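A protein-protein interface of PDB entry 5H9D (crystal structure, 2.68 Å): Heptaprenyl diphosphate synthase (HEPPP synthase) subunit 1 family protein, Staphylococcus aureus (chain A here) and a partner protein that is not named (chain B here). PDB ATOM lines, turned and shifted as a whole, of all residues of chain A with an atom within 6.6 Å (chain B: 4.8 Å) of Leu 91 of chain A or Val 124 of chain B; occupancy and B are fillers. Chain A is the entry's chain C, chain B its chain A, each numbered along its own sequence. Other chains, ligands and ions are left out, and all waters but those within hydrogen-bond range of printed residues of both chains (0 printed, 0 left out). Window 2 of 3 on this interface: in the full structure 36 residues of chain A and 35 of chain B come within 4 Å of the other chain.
SD of Met 122 of chain B sits at hydrogen-bond distance from ND2 of Asn 95 of chain A, 2.9 Å away.
CD2 of Leu 91 of chain A touches CE of Met 122 of chain B, 3.3 Å away. Val 124 of chain B touches Leu 91 of chain A. Gln 94 of chain A touches Met 122 of chain B (OE1 to CB, 3.4 Å).
Leu 91 of chain A touches just these residues of chain B: Met 122 (3.3 Å) and Val 124 (3.9 Å). Of chain A, only Leu 91 (3.9 Å) comes within 4 Å of Val 124 of chain B. Printed residues of chain B within 4 Å of Asn 95 of chain A: Met 122. Of the printed residues of chain A, Met 122 of chain B touches Leu 91, Gln 94 and Asn 95. Of the printed residues of chain B, Gln 94 of chain A touches Met 122 (3.4 Å). Lys 125 of chain B touches none of the printed residues of chain A. Asp 126 of chain B touches none of the printed residues of chain A. The nearest printed residue of chain A that does not touch Val 124 of chain B is Gln 94 of chain A (6.9 Å). The nearest printed residue of chain B that does not touch Asn 95 of chain A is Ala 123 of chain B (8.1 Å).
Of the 10 printed residues of chain B, 2 touch a printed residue of chain A. Along chain B the printed residues that touch a printed residue of chain A span positions 122 to 124. Printed residues of chain A that touch a printed residue of chain B: Leu 91, Gln 94 and Asn 95.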
ATOM      1  N   LEU A  85     -32.393  14.561  24.645  1.00  0.00           N
ATOM      2  CA  LEU A  85     -31.282  13.836  25.256  1.00  0.00           C
ATOM      3  C   LEU A  85     -30.672  14.828  26.244  1.00  0.00           C
ATOM      4  O   LEU A  85     -30.147  14.448  27.291  1.00  0.00           O
ATOM      5  CB  LEU A  85     -30.207  13.446  24.235  1.00  0.00           C
ATOM      6  CG  LEU A  85     -30.436  12.407  23.135  1.00  0.00           C
ATOM      7  CD1 LEU A  85     -29.090  12.121  22.521  1.00  0.00           C
ATOM      8  CD2 LEU A  85     -31.068  11.108  23.661  1.00  0.00           C
ATOM      9  N   ILE A  88     -32.411  14.780  29.585  1.00  0.00           N
ATOM     10  CA  ILE A  88     -32.215  13.471  30.212  1.00  0.00           C
ATOM     11  C   ILE A  88     -30.894  13.450  31.008  1.00  0.00           C
ATOM     12  O   ILE A  88     -30.674  12.608  31.876  1.00  0.00           O
ATOM     13  CB  ILE A  88     -32.223  12.341  29.159  1.00  0.00           C
ATOM     14  CG1 ILE A  88     -33.639  12.164  28.615  1.00  0.00           C
ATOM     15  CG2 ILE A  88     -31.745  11.044  29.772  1.00  0.00           C
ATOM     16  CD1 ILE A  88     -33.821  10.983  27.675  1.00  0.00           C
ATOM     17  N   ASN A  89     -30.008  14.381  30.694  1.00  0.00           N
ATOM     18  CA  ASN A  89     -28.751  14.531  31.409  1.00  0.00           C
ATOM     19  C   ASN A  89     -27.867  13.299  31.575  1.00  0.00           C
ATOM     20  O   ASN A  89     -26.716  13.427  32.001  1.00  0.00           O
ATOM     21  CB  ASN A  89     -29.039  15.123  32.782  1.00  0.00           C
ATOM     22  CG  ASN A  89     -27.921  16.008  33.280  1.00  0.00           C
ATOM     23  OD1 ASN A  89     -26.736  15.647  33.232  1.00  0.00           O
ATOM     24  ND2 ASN A  89     -28.296  17.178  33.777  1.00  0.00           N
ATOM     25  N   ASP A  90     -28.394  12.114  31.279  1.00  0.00           N
ATOM     26  CA  ASP A  90     -27.590  10.892  31.372  1.00  0.00           C
ATOM     27  C   ASP A  90     -26.647  10.906  30.171  1.00  0.00           C
ATOM     28  O   ASP A  90     -27.021  10.501  29.069  1.00  0.00           O
ATOM     29  CB  ASP A  90     -28.469   9.645  31.289  1.00  0.00           C
ATOM     30  CG  ASP A  90     -27.652   8.357  31.243  1.00  0.00           C
ATOM     31  OD1 ASP A  90     -26.498   8.385  30.743  1.00  0.00           O
ATOM     32  OD2 ASP A  90     -28.174   7.313  31.694  1.00  0.00           O
ATOM     33  N   LEU A  91     -25.423  11.358  30.380  1.00  0.00           N
ATOM     34  CA  LEU A  91     -24.483  11.446  29.281  1.00  0.00           C
ATOM     35  C   LEU A  91     -24.127  10.126  28.588  1.00  0.00           C
ATOM     36  O   LEU A  91     -24.080  10.078  27.360  1.00  0.00           O
ATOM     37  CB  LEU A  91     -23.220  12.167  29.748  1.00  0.00           C
ATOM     38  CG  LEU A  91     -22.312  12.576  28.602  1.00  0.00           C
ATOM     39  CD1 LEU A  91     -21.409  13.708  29.057  1.00  0.00           C
ATOM     40  CD2 LEU A  91     -21.515  11.369  28.150  1.00  0.00           C
ATOM     41  N   SER A  92     -23.874   9.062  29.347  1.00  0.00           N
ATOM     42  CA  SER A  92     -23.527   7.774  28.733  1.00  0.00           C
ATOM     43  C   SER A  92     -24.609   7.232  27.814  1.00  0.00           C
ATOM     44  O   SER A  92     -24.305   6.516  26.860  1.00  0.00           O
ATOM     45  CB  SER A  92     -23.216   6.716  29.795  1.00  0.00           C
ATOM     46  OG  SER A  92     -21.814   6.552  29.922  1.00  0.00           O
ATOM     47  N   PHE A  93     -25.865   7.560  28.117  1.00  0.00           N
ATOM     48  CA  PHE A  93     -26.997   7.115  27.317  1.00  0.00           C
ATOM     49  C   PHE A  93     -26.916   7.733  25.935  1.00  0.00           C
ATOM     50  O   PHE A  93     -27.349   7.123  24.953  1.00  0.00           O
ATOM     51  CB  PHE A  93     -28.308   7.517  27.989  1.00  0.00           C
ATOM     52  CG  PHE A  93     -29.525   7.313  27.131  1.00  0.00           C
ATOM     53  CD1 PHE A  93     -29.721   6.120  26.447  1.00  0.00           C
ATOM     54  CD2 PHE A  93     -30.487   8.306  27.029  1.00  0.00           C
ATOM     55  CE1 PHE A  93     -30.867   5.915  25.669  1.00  0.00           C
ATOM     56  CE2 PHE A  93     -31.631   8.121  26.263  1.00  0.00           C
ATOM     57  CZ  PHE A  93     -31.825   6.920  25.578  1.00  0.00           C
ATOM     58  N   GLN A  94     -26.352   8.940  25.866  1.00  0.00           N
ATOM     59  CA  GLN A  94     -26.205   9.638  24.595  1.00  0.00           C
ATOM     60  C   GLN A  94     -25.163   8.997  23.667  1.00  0.00           C
ATOM     61  O   GLN A  94     -25.199   9.213  22.451  1.00  0.00           O
ATOM     62  CB  GLN A  94     -25.845  11.104  24.806  1.00  0.00           C
ATOM     63  CG  GLN A  94     -25.999  11.894  23.511  1.00  0.00           C
ATOM     64  CD  GLN A  94     -25.251  13.206  23.515  1.00  0.00           C
ATOM     65  OE1 GLN A  94     -24.016  13.230  23.492  1.00  0.00           O
ATOM     66  NE2 GLN A  94     -25.993  14.312  23.545  1.00  0.00           N
ATOM     67  N   ASN A  95     -24.242   8.229  24.250  1.00  0.00           N
ATOM     68  CA  ASN A  95     -23.188   7.529  23.513  1.00  0.00           C
ATOM     69  C   ASN A  95     -23.881   6.327  22.906  1.00  0.00           C
ATOM     70  O   ASN A  95     -24.076   6.253  21.687  1.00  0.00           O
ATOM     71  CB  ASN A  95     -22.075   7.083  24.485  1.00  0.00           C
ATOM     72  CG  ASN A  95     -20.882   6.362  23.786  1.00  0.00           C
ATOM     73  OD1 ASN A  95     -20.705   5.153  23.952  1.00  0.00           O
ATOM     74  ND2 ASN A  95     -20.060   7.109  23.035  1.00  0.00           N
ATOM     75  N   GLU A  96     -24.277   5.400  23.771  1.00  0.00           N
ATOM     76  CA  GLU A  96     -24.976   4.186  23.355  1.00  0.00           C
ATOM     77  C   GLU A  96     -26.037   4.460  22.297  1.00  0.00           C
ATOM     78  O   GLU A  96     -26.141   3.750  21.299  1.00  0.00           O
ATOM     79  CB  GLU A  96     -25.661   3.544  24.562  1.00  0.00           C
ATOM     80  CG  GLU A  96     -24.717   3.002  25.609  1.00  0.00           C
ATOM     81  CD  GLU A  96     -24.149   1.648  25.203  1.00  0.00           C
ATOM     82  OE1 GLU A  96     -23.336   1.611  24.239  1.00  0.00           O
ATOM     83  OE2 GLU A  96     -24.527   0.622  25.839  1.00  0.00           O
ATOM     84  N   GLN B  63     -10.395  18.018  23.851  1.00  0.00           N
ATOM     85  CA  GLN B  63     -11.801  18.352  23.990  1.00  0.00           C
ATOM     86  C   GLN B  63     -12.227  19.449  23.020  1.00  0.00           C
ATOM     87  O   GLN B  63     -13.375  19.454  22.561  1.00  0.00           O
ATOM     88  CB  GLN B  63     -12.115  18.797  25.430  1.00  0.00           C
ATOM     89  CG  GLN B  63     -13.454  19.516  25.542  1.00  0.00           C
ATOM     90  CD  GLN B  63     -13.890  19.796  26.954  1.00  0.00           C
ATOM     91  OE1 GLN B  63     -14.884  20.473  27.176  1.00  0.00           O
ATOM     92  NE2 GLN B  63     -13.166  19.266  27.912  1.00  0.00           N
ATOM     93  N   VAL B  67     -14.866  19.284  19.635  1.00  0.00           N
ATOM     94  CA  VAL B  67     -16.043  20.099  19.363  1.00  0.00           C
ATOM     95  C   VAL B  67     -15.916  20.649  17.942  1.00  0.00           C
ATOM     96  O   VAL B  67     -16.892  20.823  17.224  1.00  0.00           O
ATOM     97  CB  VAL B  67     -16.205  21.239  20.412  1.00  0.00           C
ATOM     98  CG1 VAL B  67     -17.476  22.018  20.144  1.00  0.00           C
ATOM     99  CG2 VAL B  67     -16.291  20.632  21.789  1.00  0.00           C
ATOM    100  N   LEU B 121     -19.964  15.412  20.431  1.00  0.00           N
ATOM    101  CA  LEU B 121     -20.267  16.467  21.389  1.00  0.00           C
ATOM    102  C   LEU B 121     -20.275  15.923  22.812  1.00  0.00           C
ATOM    103  O   LEU B 121     -20.230  16.704  23.762  1.00  0.00           O
ATOM    104  CB  LEU B 121     -21.624  17.090  21.092  1.00  0.00           C
ATOM    105  CG  LEU B 121     -21.613  18.091  19.950  1.00  0.00           C
ATOM    106  CD1 LEU B 121     -23.045  18.473  19.551  1.00  0.00           C
ATOM    107  CD2 LEU B 121     -20.828  19.296  20.392  1.00  0.00           C
ATOM    108  N   MET B 122     -20.332  14.596  22.956  1.00  0.00           N
ATOM    109  CA  MET B 122     -20.348  13.973  24.287  1.00  0.00           C
ATOM    110  C   MET B 122     -18.971  14.056  24.933  1.00  0.00           C
ATOM    111  O   MET B 122     -18.718  13.413  25.959  1.00  0.00           O
ATOM    112  CB  MET B 122     -20.783  12.499  24.226  1.00  0.00           C
ATOM    113  CG  MET B 122     -19.630  11.497  24.035  1.00  0.00           C
ATOM    114  SD  MET B 122     -20.220   9.797  24.000  1.00  0.00           S
ATOM    115  CE  MET B 122     -20.405   9.459  25.764  1.00  0.00           C
ATOM    116  N   ALA B 123     -18.082  14.828  24.304  1.00  0.00           N
ATOM    117  CA  ALA B 123     -16.730  15.041  24.805  1.00  0.00           C
ATOM    118  C   ALA B 123     -16.804  16.308  25.652  1.00  0.00           C
ATOM    119  O   ALA B 123     -15.901  16.629  26.421  1.00  0.00           O
ATOM    120  CB  ALA B 123     -15.753  15.216  23.649  1.00  0.00           C
ATOM    121  N   VAL B 124     -17.883  17.051  25.484  1.00  0.00           N
ATOM    122  CA  VAL B 124     -18.089  18.239  26.279  1.00  0.00           C
ATOM    123  C   VAL B 124     -18.769  17.623  27.500  1.00  0.00           C
ATOM    124  O   VAL B 124     -19.509  16.644  27.366  1.00  0.00           O
ATOM    125  CB  VAL B 124     -19.048  19.220  25.579  1.00  0.00           C
ATOM    126  CG1 VAL B 124     -19.281  20.441  26.462  1.00  0.00           C
ATOM    127  CG2 VAL B 124     -18.471  19.633  24.233  1.00  0.00           C
ATOM    128  N   LYS B 125     -18.525  18.182  28.680  1.00  0.00           N
ATOM    129  CA  LYS B 125     -19.098  17.622  29.901  1.00  0.00           C
ATOM    130  C   LYS B 125     -20.239  18.443  30.494  1.00  0.00           C
ATOM    131  O   LYS B 125     -21.124  17.903  31.157  1.00  0.00           O
ATOM    132  CB  LYS B 125     -17.987  17.432  30.944  1.00  0.00           C
ATOM    133  CG  LYS B 125     -16.694  16.798  30.381  1.00  0.00           C
ATOM    134  CD  LYS B 125     -15.879  17.801  29.525  1.00  0.00           C
ATOM    135  CE  LYS B 125     -15.194  18.894  30.362  1.00  0.00           C
ATOM    136  NZ  LYS B 125     -13.938  18.449  31.066  1.00  0.00           N
ATOM    137  N   ASP B 126     -20.225  19.747  30.240  1.00  0.00           N
ATOM    138  CA  ASP B 126     -21.255  20.649  30.758  1.00  0.00           C
ATOM    139  C   ASP B 126     -22.619  20.458  30.076  1.00  0.00           C
ATOM    140  O   ASP B 126     -22.798  20.833  28.918  1.00  0.00           O
ATOM    141  CB  ASP B 126     -20.789  22.092  30.582  1.00  0.00           C
ATOM    142  CG  ASP B 126     -21.497  23.045  31.506  1.00  0.00           C
ATOM    143  OD1 ASP B 126     -22.745  22.995  31.574  1.00  0.00           O
ATOM    144  OD2 ASP B 126     -20.798  23.849  32.161  1.00  0.00           O
ATOM    145  N   VAL B 129     -24.240  23.147  27.805  1.00  0.00           N
ATOM    146  CA  VAL B 129     -23.759  23.386  26.447  1.00  0.00           C
ATOM    147  C   VAL B 129     -24.684  22.579  25.525  1.00  0.00           C
ATOM    148  O   VAL B 129     -25.216  23.103  24.543  1.00  0.00           O
ATOM    149  CB  VAL B 129     -22.285  22.896  26.268  1.00  0.00           C
ATOM    150  CG1 VAL B 129     -22.033  22.472  24.829  1.00  0.00           C
ATOM    151  CG2 VAL B 129     -21.326  23.993  26.649  1.00  0.00           C
ATOM    152  N   HIS B 130     -24.876  21.306  25.870  1.00  0.00           N
ATOM    153  CA  HIS B 130     -25.730  20.397  25.109  1.00  0.00           C
ATOM    154  C   HIS B 130     -27.140  20.951  24.952  1.00  0.00           C
ATOM    155  O   HIS B 130     -27.737  20.847  23.879  1.00  0.00           O
ATOM    156  CB  HIS B 130     -25.776  19.022  25.784  1.00  0.00           C
ATOM    157  CG  HIS B 130     -24.522  18.227  25.615  1.00  0.00           C
ATOM    158  ND1 HIS B 130     -24.098  17.764  24.391  1.00  0.00           N
ATOM    159  CD2 HIS B 130     -23.579  17.847  26.504  1.00  0.00           C
ATOM    160  CE1 HIS B 130     -22.946  17.136  24.531  1.00  0.00           C
ATOM    161  NE2 HIS B 130     -22.607  17.175  25.805  1.00  0.00           N
